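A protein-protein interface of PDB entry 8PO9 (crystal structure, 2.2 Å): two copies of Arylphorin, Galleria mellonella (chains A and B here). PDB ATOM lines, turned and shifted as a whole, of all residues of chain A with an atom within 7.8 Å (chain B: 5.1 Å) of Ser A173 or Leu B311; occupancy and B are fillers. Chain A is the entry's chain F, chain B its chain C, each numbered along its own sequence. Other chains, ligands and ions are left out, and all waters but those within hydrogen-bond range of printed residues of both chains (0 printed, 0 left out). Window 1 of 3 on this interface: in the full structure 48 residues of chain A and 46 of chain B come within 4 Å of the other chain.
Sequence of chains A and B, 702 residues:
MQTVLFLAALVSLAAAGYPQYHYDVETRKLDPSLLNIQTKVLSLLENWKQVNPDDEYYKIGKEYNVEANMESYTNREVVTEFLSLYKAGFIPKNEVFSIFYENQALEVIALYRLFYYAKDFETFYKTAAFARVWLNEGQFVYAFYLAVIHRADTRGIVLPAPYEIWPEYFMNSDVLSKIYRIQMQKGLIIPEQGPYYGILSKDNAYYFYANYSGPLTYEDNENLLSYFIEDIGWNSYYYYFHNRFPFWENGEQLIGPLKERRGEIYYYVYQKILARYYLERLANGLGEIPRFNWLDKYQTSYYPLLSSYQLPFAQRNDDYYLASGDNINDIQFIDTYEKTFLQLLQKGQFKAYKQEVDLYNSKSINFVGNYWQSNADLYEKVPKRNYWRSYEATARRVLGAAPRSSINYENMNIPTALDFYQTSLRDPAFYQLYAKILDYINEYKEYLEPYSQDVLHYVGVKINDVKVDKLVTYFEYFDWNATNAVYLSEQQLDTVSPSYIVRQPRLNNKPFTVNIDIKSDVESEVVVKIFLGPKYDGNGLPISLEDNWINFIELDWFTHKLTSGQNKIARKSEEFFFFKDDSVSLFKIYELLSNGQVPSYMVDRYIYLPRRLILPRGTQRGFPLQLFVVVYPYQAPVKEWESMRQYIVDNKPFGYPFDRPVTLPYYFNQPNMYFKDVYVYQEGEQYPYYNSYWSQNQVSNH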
ATOM      1  N   GLU A 168      -9.126  13.536 -27.855  1.00  0.00           N
ATOM      2  CA  GLU A 168      -9.329  14.932 -27.488  1.00  0.00           C
ATOM      3  C   GLU A 168      -8.881  15.232 -26.058  1.00  0.00           C
ATOM      4  O   GLU A 168      -8.663  16.402 -25.710  1.00  0.00           O
ATOM      5  CB  GLU A 168     -10.791  15.310 -27.667  1.00  0.00           C
ATOM      6  CG  GLU A 168     -11.767  14.602 -26.771  1.00  0.00           C
ATOM      7  CD  GLU A 168     -12.239  13.233 -27.249  1.00  0.00           C
ATOM      8  OE1 GLU A 168     -11.712  12.660 -28.236  1.00  0.00           O
ATOM      9  OE2 GLU A 168     -13.191  12.732 -26.608  1.00  0.00           O
ATOM     10  N   MET A 171      -4.237  15.570 -26.225  1.00  0.00           N
ATOM     11  CA  MET A 171      -3.422  16.511 -26.984  1.00  0.00           C
ATOM     12  C   MET A 171      -3.970  17.912 -26.754  1.00  0.00           C
ATOM     13  O   MET A 171      -5.123  18.084 -26.351  1.00  0.00           O
ATOM     14  CB  MET A 171      -3.418  16.154 -28.474  1.00  0.00           C
ATOM     15  CG  MET A 171      -4.745  16.470 -29.158  1.00  0.00           C
ATOM     16  SD  MET A 171      -4.774  16.029 -30.896  1.00  0.00           S
ATOM     17  CE  MET A 171      -5.504  14.391 -30.791  1.00  0.00           C
ATOM     18  N   ASN A 172      -3.153  18.920 -27.033  1.00  0.00           N
ATOM     19  CA  ASN A 172      -3.634  20.282 -26.855  1.00  0.00           C
ATOM     20  C   ASN A 172      -4.477  20.744 -28.049  1.00  0.00           C
ATOM     21  O   ASN A 172      -4.433  20.165 -29.142  1.00  0.00           O
ATOM     22  CB  ASN A 172      -2.479  21.247 -26.653  1.00  0.00           C
ATOM     23  CG  ASN A 172      -1.855  21.122 -25.294  1.00  0.00           C
ATOM     24  OD1 ASN A 172      -2.490  20.653 -24.337  1.00  0.00           O
ATOM     25  ND2 ASN A 172      -0.606  21.584 -25.178  1.00  0.00           N
ATOM     26  N   SER A 173      -5.225  21.835 -27.828  1.00  0.00           N
ATOM     27  CA  SER A 173      -6.161  22.352 -28.825  1.00  0.00           C
ATOM     28  C   SER A 173      -5.469  22.879 -30.083  1.00  0.00           C
ATOM     29  O   SER A 173      -6.122  22.985 -31.119  1.00  0.00           O
ATOM     30  CB  SER A 173      -7.044  23.459 -28.225  1.00  0.00           C
ATOM     31  OG  SER A 173      -6.304  24.650 -27.976  1.00  0.00           O
ATOM     32  N   ASP A 174      -4.186  23.259 -30.013  1.00  0.00           N
ATOM     33  CA  ASP A 174      -3.510  23.699 -31.229  1.00  0.00           C
ATOM     34  C   ASP A 174      -3.298  22.537 -32.202  1.00  0.00           C
ATOM     35  O   ASP A 174      -3.366  22.734 -33.415  1.00  0.00           O
ATOM     36  CB  ASP A 174      -2.190  24.414 -30.901  1.00  0.00           C
ATOM     37  CG  ASP A 174      -1.165  23.511 -30.245  1.00  0.00           C
ATOM     38  OD1 ASP A 174      -1.517  22.761 -29.312  1.00  0.00           O
ATOM     39  OD2 ASP A 174       0.013  23.545 -30.670  1.00  0.00           O
ATOM     40  N   VAL A 175      -3.046  21.330 -31.696  1.00  0.00           N
ATOM     41  CA  VAL A 175      -2.984  20.152 -32.553  1.00  0.00           C
ATOM     42  C   VAL A 175      -4.376  19.764 -33.044  1.00  0.00           C
ATOM     43  O   VAL A 175      -4.571  19.436 -34.225  1.00  0.00           O
ATOM     44  CB  VAL A 175      -2.317  18.980 -31.809  1.00  0.00           C
ATOM     45  CG1 VAL A 175      -2.014  17.824 -32.793  1.00  0.00           C
ATOM     46  CG2 VAL A 175      -1.067  19.445 -31.124  1.00  0.00           C
ATOM     47  N   LEU A 176      -5.354  19.739 -32.132  1.00  0.00           N
ATOM     48  CA  LEU A 176      -6.713  19.327 -32.495  1.00  0.00           C
ATOM     49  C   LEU A 176      -7.320  20.246 -33.557  1.00  0.00           C
ATOM     50  O   LEU A 176      -8.072  19.793 -34.436  1.00  0.00           O
ATOM     51  CB  LEU A 176      -7.590  19.302 -31.243  1.00  0.00           C
ATOM     52  CG  LEU A 176      -8.121  17.969 -30.727  1.00  0.00           C
ATOM     53  CD1 LEU A 176      -9.222  18.227 -29.720  1.00  0.00           C
ATOM     54  CD2 LEU A 176      -8.629  17.098 -31.845  1.00  0.00           C
ATOM     55  N   SER A 177      -7.079  21.550 -33.444  1.00  0.00           N
ATOM     56  CA  SER A 177      -7.654  22.467 -34.417  1.00  0.00           C
ATOM     57  C   SER A 177      -7.107  22.217 -35.818  1.00  0.00           C
ATOM     58  O   SER A 177      -7.823  22.416 -36.805  1.00  0.00           O
ATOM     59  CB  SER A 177      -7.431  23.916 -33.971  1.00  0.00           C
ATOM     60  OG  SER A 177      -6.082  24.316 -34.073  1.00  0.00           O
ATOM     61  N   LYS A 178      -5.837  21.818 -35.930  1.00  0.00           N
ATOM     62  CA  LYS A 178      -5.296  21.429 -37.230  1.00  0.00           C
ATOM     63  C   LYS A 178      -6.001  20.192 -37.766  1.00  0.00           C
ATOM     64  O   LYS A 178      -6.307  20.102 -38.961  1.00  0.00           O
ATOM     65  CB  LYS A 178      -3.797  21.145 -37.133  1.00  0.00           C
ATOM     66  CG  LYS A 178      -2.903  22.355 -36.905  1.00  0.00           C
ATOM     67  CD  LYS A 178      -1.494  21.876 -36.689  1.00  0.00           C
ATOM     68  CE  LYS A 178      -0.522  23.021 -36.629  1.00  0.00           C
ATOM     69  NZ  LYS A 178       0.839  22.491 -36.356  1.00  0.00           N
ATOM     70  N   ILE A 179      -6.245  19.217 -36.894  1.00  0.00           N
ATOM     71  CA  ILE A 179      -6.897  17.983 -37.306  1.00  0.00           C
ATOM     72  C   ILE A 179      -8.317  18.265 -37.779  1.00  0.00           C
ATOM     73  O   ILE A 179      -8.737  17.782 -38.835  1.00  0.00           O
ATOM     74  CB  ILE A 179      -6.853  16.961 -36.159  1.00  0.00           C
ATOM     75  CG1 ILE A 179      -5.395  16.542 -35.902  1.00  0.00           C
ATOM     76  CG2 ILE A 179      -7.659  15.770 -36.498  1.00  0.00           C
ATOM     77  CD1 ILE A 179      -5.218  15.573 -34.716  1.00  0.00           C
ATOM     78  N   TYR A 180      -9.069  19.076 -37.017  1.00  0.00           N
ATOM     79  CA  TYR A 180     -10.428  19.444 -37.416  1.00  0.00           C
ATOM     80  C   TYR A 180     -10.443  20.189 -38.745  1.00  0.00           C
ATOM     81  O   TYR A 180     -11.329  19.967 -39.581  1.00  0.00           O
ATOM     82  CB  TYR A 180     -11.091  20.313 -36.347  1.00  0.00           C
ATOM     83  CG  TYR A 180     -11.362  19.664 -35.012  1.00  0.00           C
ATOM     84  CD1 TYR A 180     -11.616  18.309 -34.912  1.00  0.00           C
ATOM     85  CD2 TYR A 180     -11.395  20.426 -33.851  1.00  0.00           C
ATOM     86  CE1 TYR A 180     -11.888  17.721 -33.695  1.00  0.00           C
ATOM     87  CE2 TYR A 180     -11.665  19.852 -32.642  1.00  0.00           C
ATOM     88  CZ  TYR A 180     -11.916  18.491 -32.570  1.00  0.00           C
ATOM     89  OH  TYR A 180     -12.177  17.901 -31.351  1.00  0.00           O
ATOM     90  N   SER A 213       2.780  21.226 -23.833  1.00  0.00           N
ATOM     91  CA  SER A 213       2.470  22.585 -23.417  1.00  0.00           C
ATOM     92  C   SER A 213       3.749  23.330 -23.044  1.00  0.00           C
ATOM     93  O   SER A 213       4.766  22.728 -22.673  1.00  0.00           O
ATOM     94  CB  SER A 213       1.512  22.569 -22.225  1.00  0.00           C
ATOM     95  OG  SER A 213       0.274  21.948 -22.540  1.00  0.00           O
ATOM     96  N   LEU A 216       2.849  29.094 -21.344  1.00  0.00           N
ATOM     97  CA  LEU A 216       1.482  29.616 -21.246  1.00  0.00           C
ATOM     98  C   LEU A 216       0.648  28.784 -20.278  1.00  0.00           C
ATOM     99  O   LEU A 216      -0.110  29.325 -19.463  1.00  0.00           O
ATOM    100  CB  LEU A 216       0.792  29.618 -22.614  1.00  0.00           C
ATOM    101  CG  LEU A 216       1.205  30.577 -23.732  1.00  0.00           C
ATOM    102  CD1 LEU A 216       0.350  30.301 -24.993  1.00  0.00           C
ATOM    103  CD2 LEU A 216       1.098  32.029 -23.306  1.00  0.00           C
ATOM    104  N   THR A 217       0.804  27.468 -20.333  1.00  0.00           N
ATOM    105  CA  THR A 217      -0.018  26.575 -19.530  1.00  0.00           C
ATOM    106  C   THR A 217       0.517  26.437 -18.108  1.00  0.00           C
ATOM    107  O   THR A 217      -0.260  26.470 -17.146  1.00  0.00           O
ATOM    108  CB  THR A 217      -0.083  25.226 -20.229  1.00  0.00           C
ATOM    109  OG1 THR A 217      -0.791  25.394 -21.464  1.00  0.00           O
ATOM    110  CG2 THR A 217      -0.797  24.173 -19.371  1.00  0.00           C
ATOM    111  N   PRO A 304      -4.830  25.221 -19.119  1.00  0.00           N
ATOM    112  CA  PRO A 304      -4.812  24.125 -20.100  1.00  0.00           C
ATOM    113  C   PRO A 304      -5.304  24.566 -21.477  1.00  0.00           C
ATOM    114  O   PRO A 304      -6.272  25.314 -21.608  1.00  0.00           O
ATOM    115  CB  PRO A 304      -5.745  23.075 -19.478  1.00  0.00           C
ATOM    116  CG  PRO A 304      -6.682  23.902 -18.591  1.00  0.00           C
ATOM    117  CD  PRO A 304      -5.823  25.005 -18.049  1.00  0.00           C
ATOM    118  N   LEU A 305      -4.637  24.060 -22.511  1.00  0.00           N
ATOM    119  CA  LEU A 305      -5.086  24.210 -23.887  1.00  0.00           C
ATOM    120  C   LEU A 305      -5.881  22.986 -24.288  1.00  0.00           C
ATOM    121  O   LEU A 305      -5.693  22.413 -25.349  1.00  0.00           O
ATOM    122  CB  LEU A 305      -3.908  24.433 -24.822  1.00  0.00           C
ATOM    123  CG  LEU A 305      -2.979  25.572 -24.418  1.00  0.00           C
ATOM    124  CD1 LEU A 305      -1.904  25.748 -25.463  1.00  0.00           C
ATOM    125  CD2 LEU A 305      -3.726  26.874 -24.224  1.00  0.00           C
ATOM    126  N   LEU A 306      -6.701  22.519 -23.365  1.00  0.00           N
ATOM    127  CA  LEU A 306      -7.603  21.400 -23.550  1.00  0.00           C
ATOM    128  C   LEU A 306      -9.012  21.941 -23.690  1.00  0.00           C
ATOM    129  O   LEU A 306      -9.346  22.988 -23.124  1.00  0.00           O
ATOM    130  CB  LEU A 306      -7.550  20.445 -22.353  1.00  0.00           C
ATOM    131  CG  LEU A 306      -6.188  19.814 -22.120  1.00  0.00           C
ATOM    132  CD1 LEU A 306      -6.034  19.376 -20.657  1.00  0.00           C
ATOM    133  CD2 LEU A 306      -6.066  18.649 -23.056  1.00  0.00           C
ATOM    134  N   SER A 307      -9.832  21.228 -24.450  1.00  0.00           N
ATOM    135  CA  SER A 307     -11.248  21.543 -24.503  1.00  0.00           C
ATOM    136  C   SER A 307     -12.034  20.244 -24.602  1.00  0.00           C
ATOM    137  O   SER A 307     -11.505  19.192 -24.967  1.00  0.00           O
ATOM    138  CB  SER A 307     -11.628  22.453 -25.683  1.00  0.00           C
ATOM    139  OG  SER A 307     -11.813  21.714 -26.871  1.00  0.00           O
ATOM    140  N   PRO A 312     -14.409  25.253 -23.464  1.00  0.00           N
ATOM    141  CA  PRO A 312     -13.015  25.167 -23.025  1.00  0.00           C
ATOM    142  C   PRO A 312     -12.913  24.554 -21.636  1.00  0.00           C
ATOM    143  O   PRO A 312     -13.853  24.596 -20.843  1.00  0.00           O
ATOM    144  CB  PRO A 312     -12.575  26.629 -22.998  1.00  0.00           C
ATOM    145  CG  PRO A 312     -13.807  27.345 -22.630  1.00  0.00           C
ATOM    146  CD  PRO A 312     -14.919  26.632 -23.356  1.00  0.00           C
ATOM    147  N   GLN A 315      -9.649  27.462 -16.548  1.00  0.00           N
ATOM    148  CA  GLN A 315      -8.312  27.945 -16.233  1.00  0.00           C
ATOM    149  C   GLN A 315      -8.273  28.458 -14.799  1.00  0.00           C
ATOM    150  O   GLN A 315      -9.236  29.057 -14.331  1.00  0.00           O
ATOM    151  CB  GLN A 315      -7.906  29.062 -17.207  1.00  0.00           C
ATOM    152  CG  GLN A 315      -8.085  28.661 -18.660  1.00  0.00           C
ATOM    153  CD  GLN A 315      -8.221  29.847 -19.603  1.00  0.00           C
ATOM    154  OE1 GLN A 315      -7.907  30.996 -19.244  1.00  0.00           O
ATOM    155  NE2 GLN A 315      -8.723  29.578 -20.812  1.00  0.00           N
ATOM    156  N   ARG A 426      -2.376  16.016 -15.682  1.00  0.00           N
ATOM    157  CA  ARG A 426      -1.828  17.212 -16.317  1.00  0.00           C
ATOM    158  C   ARG A 426      -1.820  18.429 -15.398  1.00  0.00           C
ATOM    159  O   ARG A 426      -1.013  19.345 -15.607  1.00  0.00           O
ATOM    160  CB  ARG A 426      -2.623  17.554 -17.577  1.00  0.00           C
ATOM    161  CG  ARG A 426      -2.524  16.528 -18.701  1.00  0.00           C
ATOM    162  CD  ARG A 426      -3.411  16.956 -19.860  1.00  0.00           C
ATOM    163  NE  ARG A 426      -3.082  16.297 -21.121  1.00  0.00           N
ATOM    164  CZ  ARG A 426      -2.530  16.902 -22.169  1.00  0.00           C
ATOM    165  NH1 ARG A 426      -2.211  18.192 -22.138  1.00  0.00           N
ATOM    166  NH2 ARG A 426      -2.345  16.212 -23.292  1.00  0.00           N
ATOM    167  N   VAL B  96      -2.696  33.590 -33.717  1.00  0.00           N
ATOM    168  CA  VAL B  96      -3.636  34.586 -33.218  1.00  0.00           C
ATOM    169  C   VAL B  96      -3.032  35.975 -33.411  1.00  0.00           C
ATOM    170  O   VAL B  96      -1.867  36.210 -33.066  1.00  0.00           O
ATOM    171  CB  VAL B  96      -3.957  34.305 -31.740  1.00  0.00           C
ATOM    172  CG1 VAL B  96      -5.050  35.214 -31.236  1.00  0.00           C
ATOM    173  CG2 VAL B  96      -4.308  32.813 -31.522  1.00  0.00           C
ATOM    174  N   SER B 307     -13.383  31.469 -28.412  1.00  0.00           N
ATOM    175  CA  SER B 307     -12.057  30.982 -28.739  1.00  0.00           C
ATOM    176  C   SER B 307     -11.618  31.606 -30.047  1.00  0.00           C
ATOM    177  O   SER B 307     -12.435  32.088 -30.838  1.00  0.00           O
ATOM    178  CB  SER B 307     -12.016  29.470 -28.881  1.00  0.00           C
ATOM    179  OG  SER B 307     -12.502  29.118 -30.150  1.00  0.00           O
ATOM    180  N   SER B 308     -10.302  31.600 -30.251  1.00  0.00           N
ATOM    181  CA  SER B 308      -9.682  31.939 -31.521  1.00  0.00           C
ATOM    182  C   SER B 308      -9.324  30.693 -32.322  1.00  0.00           C
ATOM    183  O   SER B 308      -8.378  30.706 -33.118  1.00  0.00           O
ATOM    184  CB  SER B 308      -8.449  32.794 -31.265  1.00  0.00           C
ATOM    185  OG  SER B 308      -7.560  32.030 -30.484  1.00  0.00           O
ATOM    186  N   TYR B 309     -10.056  29.607 -32.085  1.00  0.00           N
ATOM    187  CA  TYR B 309     -10.020  28.340 -32.816  1.00  0.00           C
ATOM    188  C   TYR B 309      -8.750  27.532 -32.588  1.00  0.00           C
ATOM    189  O   TYR B 309      -8.802  26.300 -32.491  1.00  0.00           O
ATOM    190  CB  TYR B 309     -10.157  28.588 -34.330  1.00  0.00           C
ATOM    191  CG  TYR B 309     -10.067  27.309 -35.117  1.00  0.00           C
ATOM    192  CD1 TYR B 309     -11.118  26.406 -35.098  1.00  0.00           C
ATOM    193  CD2 TYR B 309      -8.914  26.974 -35.839  1.00  0.00           C
ATOM    194  CE1 TYR B 309     -11.050  25.214 -35.789  1.00  0.00           C
ATOM    195  CE2 TYR B 309      -8.836  25.768 -36.547  1.00  0.00           C
ATOM    196  CZ  TYR B 309      -9.916  24.902 -36.508  1.00  0.00           C
ATOM    197  OH  TYR B 309      -9.900  23.704 -37.163  1.00  0.00           O
ATOM    198  N   GLN B 310      -7.647  28.206 -32.313  1.00  0.00           N
ATOM    199  CA  GLN B 310      -6.412  27.509 -32.013  1.00  0.00           C
ATOM    200  C   GLN B 310      -6.177  27.436 -30.514  1.00  0.00           C
ATOM    201  O   GLN B 310      -5.444  26.555 -30.053  1.00  0.00           O
ATOM    202  CB  GLN B 310      -5.228  28.210 -32.705  1.00  0.00           C
ATOM    203  CG  GLN B 310      -3.917  27.450 -32.658  1.00  0.00           C
ATOM    204  CD  GLN B 310      -2.698  28.292 -33.049  1.00  0.00           C
ATOM    205  OE1 GLN B 310      -2.606  29.478 -32.728  1.00  0.00           O
ATOM    206  NE2 GLN B 310      -1.766  27.675 -33.776  1.00  0.00           N
ATOM    207  N   LEU B 311      -6.807  28.342 -29.764  1.00  0.00           N
ATOM    208  CA  LEU B 311      -6.588  28.589 -28.349  1.00  0.00           C
ATOM    209  C   LEU B 311      -7.891  29.080 -27.738  1.00  0.00           C
ATOM    210  O   LEU B 311      -8.663  29.765 -28.416  1.00  0.00           O
ATOM    211  CB  LEU B 311      -5.485  29.639 -28.155  1.00  0.00           C
ATOM    212  CG  LEU B 311      -4.112  29.286 -28.729  1.00  0.00           C
ATOM    213  CD1 LEU B 311      -3.190  30.503 -28.814  1.00  0.00           C
ATOM    214  CD2 LEU B 311      -3.494  28.210 -27.855  1.00  0.00           C
ATOM    215  N   PRO B 312      -8.166  28.749 -26.477  1.00  0.00           N
ATOM    216  CA  PRO B 312      -9.300  29.364 -25.773  1.00  0.00           C
ATOM    217  C   PRO B 312      -9.004  30.808 -25.392  1.00  0.00           C
ATOM    218  O   PRO B 312      -7.852  31.241 -25.353  1.00  0.00           O
ATOM    219  CB  PRO B 312      -9.442  28.502 -24.519  1.00  0.00           C
ATOM    220  CG  PRO B 312      -8.035  28.046 -24.239  1.00  0.00           C
ATOM    221  CD  PRO B 312      -7.442  27.792 -25.620  1.00  0.00           C
ATOM    222  N   PHE B 313     -10.068  31.571 -25.155  1.00  0.00           N
ATOM    223  CA  PHE B 313      -9.906  32.877 -24.532  1.00  0.00           C
ATOM    224  C   PHE B 313      -9.551  32.718 -23.062  1.00  0.00           C
ATOM    225  O   PHE B 313      -9.934  31.743 -22.407  1.00  0.00           O
ATOM    226  CB  PHE B 313     -11.175  33.735 -24.676  1.00  0.00           C
ATOM    227  CG  PHE B 313     -11.272  34.502 -25.993  1.00  0.00           C
ATOM    228  CD1 PHE B 313     -10.958  33.896 -27.210  1.00  0.00           C
ATOM    229  CD2 PHE B 313     -11.702  35.820 -26.004  1.00  0.00           C
ATOM    230  CE1 PHE B 313     -11.060  34.597 -28.415  1.00  0.00           C
ATOM    231  CE2 PHE B 313     -11.807  36.539 -27.194  1.00  0.00           C
ATOM    232  CZ  PHE B 313     -11.489  35.926 -28.408  1.00  0.00           C
ATOM    233  N   ASN B 413       0.643  33.828 -27.102  1.00  0.00           N
ATOM    234  CA  ASN B 413      -0.388  34.596 -26.425  1.00  0.00           C
ATOM    235  C   ASN B 413      -1.610  33.725 -26.173  1.00  0.00           C
ATOM    236  O   ASN B 413      -2.016  32.956 -27.043  1.00  0.00           O
ATOM    237  CB  ASN B 413      -0.822  35.820 -27.260  1.00  0.00           C
ATOM    238  CG  ASN B 413       0.289  36.815 -27.474  1.00  0.00           C
ATOM    239  OD1 ASN B 413       0.644  37.559 -26.561  1.00  0.00           O
ATOM    240  ND2 ASN B 413       0.838  36.851 -28.684  1.00  0.00           N
ATOM    241  N   ILE B 414      -2.220  33.867 -24.999  1.00  0.00           N
ATOM    242  CA  ILE B 414      -3.591  33.414 -24.786  1.00  0.00           C
ATOM    243  C   ILE B 414      -4.497  34.625 -24.981  1.00  0.00           C
ATOM    244  O   ILE B 414      -4.427  35.573 -24.184  1.00  0.00           O
ATOM    245  CB  ILE B 414      -3.803  32.766 -23.412  1.00  0.00           C
ATOM    246  CG1 ILE B 414      -3.096  31.418 -23.359  1.00  0.00           C
ATOM    247  CG2 ILE B 414      -5.309  32.599 -23.093  1.00  0.00           C
ATOM    248  CD1 ILE B 414      -3.370  30.641 -22.070  1.00  0.00           C
ATOM    249  N   PRO B 415      -5.317  34.651 -26.016  1.00  0.00           N
ATOM    250  CA  PRO B 415      -6.096  35.853 -26.300  1.00  0.00           C
ATOM    251  C   PRO B 415      -7.150  36.071 -25.231  1.00  0.00           C
ATOM    252  O   PRO B 415      -7.635  35.128 -24.597  1.00  0.00           O
ATOM    253  CB  PRO B 415      -6.725  35.548 -27.663  1.00  0.00           C
ATOM    254  CG  PRO B 415      -6.810  34.037 -27.691  1.00  0.00           C
ATOM    255  CD  PRO B 415      -5.618  33.540 -26.940  1.00  0.00           C
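Ser A173 touches Leu B311 (OG to CA, 3.97 Å).
Gln B310 touches Asp A174.
Ser A177 touches Gln B310 (OG to CA, 3.8 Å).
Tyr A180 touches Tyr B309.
CD1 of Leu A216 touches CG1 of Ile B414, 3.97 Å away.
Leu A305 touches Leu B311.
CB of Pro B312 touches CB of Pro A312 (3.95 Å).
Gln A315 touches Pro B312 (NE2 to CG, 3.8 Å).
Printed residues of chain B within 4 Å of Ser A173: Gln B310 (2.9 Å) and Leu B311 (3.97 Å).
Printed residues of chain B within 4 Å of Asp A174: Gln B310.
Of the printed residues of chain B, Tyr A180 touches Tyr B309.
Printed residues of chain B within 4 Å of Leu A305: Leu B311 (3.8 Å).
Ser A307 touches none of the printed residues of chain B.
Of the printed residues of chain A, Gln B310 touches Ser A173, Asp A174 and Ser A177.
Leu B311 touches just these residues of chain A: Ser A173 and Leu A305.
Pro B312 touches just these residues of chain A: Pro A312 and Gln A315.
Of the printed residues of chain A, Phe B313 touches Gln A315.
The nearest residue of chain B that does not touch Ser A173 is Pro B312 (4.1 Å).
The side-chain hydroxyl (OG) of Ser B308 lies within hydrogen-bond range of the backbone carbonyl oxygen (O) of Leu B311, at 3.3 Å.
OG of Ser B307 sits at hydrogen-bond distance from N of Tyr B309.
The side-chain hydroxyl (OG) of Ser A177 sits at hydrogen-bond distance from the backbone carbonyl oxygen (O) of Ser A173, 3.2 Å away.
The backbone NH (N) of Ser A173 is in hydrogen-bond range of the backbone carbonyl oxygen (O) of Leu A305 (2.6 Å).
The side-chain hydroxyl (OG) of Ser A177 is in hydrogen-bond range of the backbone carbonyl oxygen (O) of Asp A174 (3.2 Å).
O of Phe B313 lies within hydrogen-bond range of NE2 of Gln A315 (2.9 Å).
The backbone carbonyl oxygen (O) of Gln B310 is in hydrogen-bond range of the side-chain hydroxyl (OG) of Ser A173.
The side-chain hydroxyl (OH) of Tyr B309 is in hydrogen-bond range of the backbone carbonyl oxygen (O) of Ser A177, at 2.5 Å.
Of the 21 printed residues of chain A, 8 touch a printed residue of chain B.
Hydrophobic or aromatic side chains of chain A within 4 Å of the printed part of chain B: Tyr A180, Leu A216, Leu A305 and Pro A312.
Along chain A the printed residues that touch a printed residue of chain B span positions 173 to 315.
Of the 11 printed residues of chain B, 6 touch a printed residue of chain A.
Hydrophobic or aromatic side chains of chain B within 4 Å of the printed part of chain A: Tyr B309, Leu B311, Pro B312 and Ile B414.
Among the printed residues, 11 pairs touch across the chains.
Among the printed residues, no Asp or Glu carboxylate lies within 4 Å of a Lys or Arg side-chain nitrogen of the other chain.
Pro B312 touches its own counterpart, Pro A312.
Positions printed for both chains: 307 and 312.
Of the 11 pairs that touch across the chains among the printed residues, 1 has its exchanged pair printed and touching as well.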
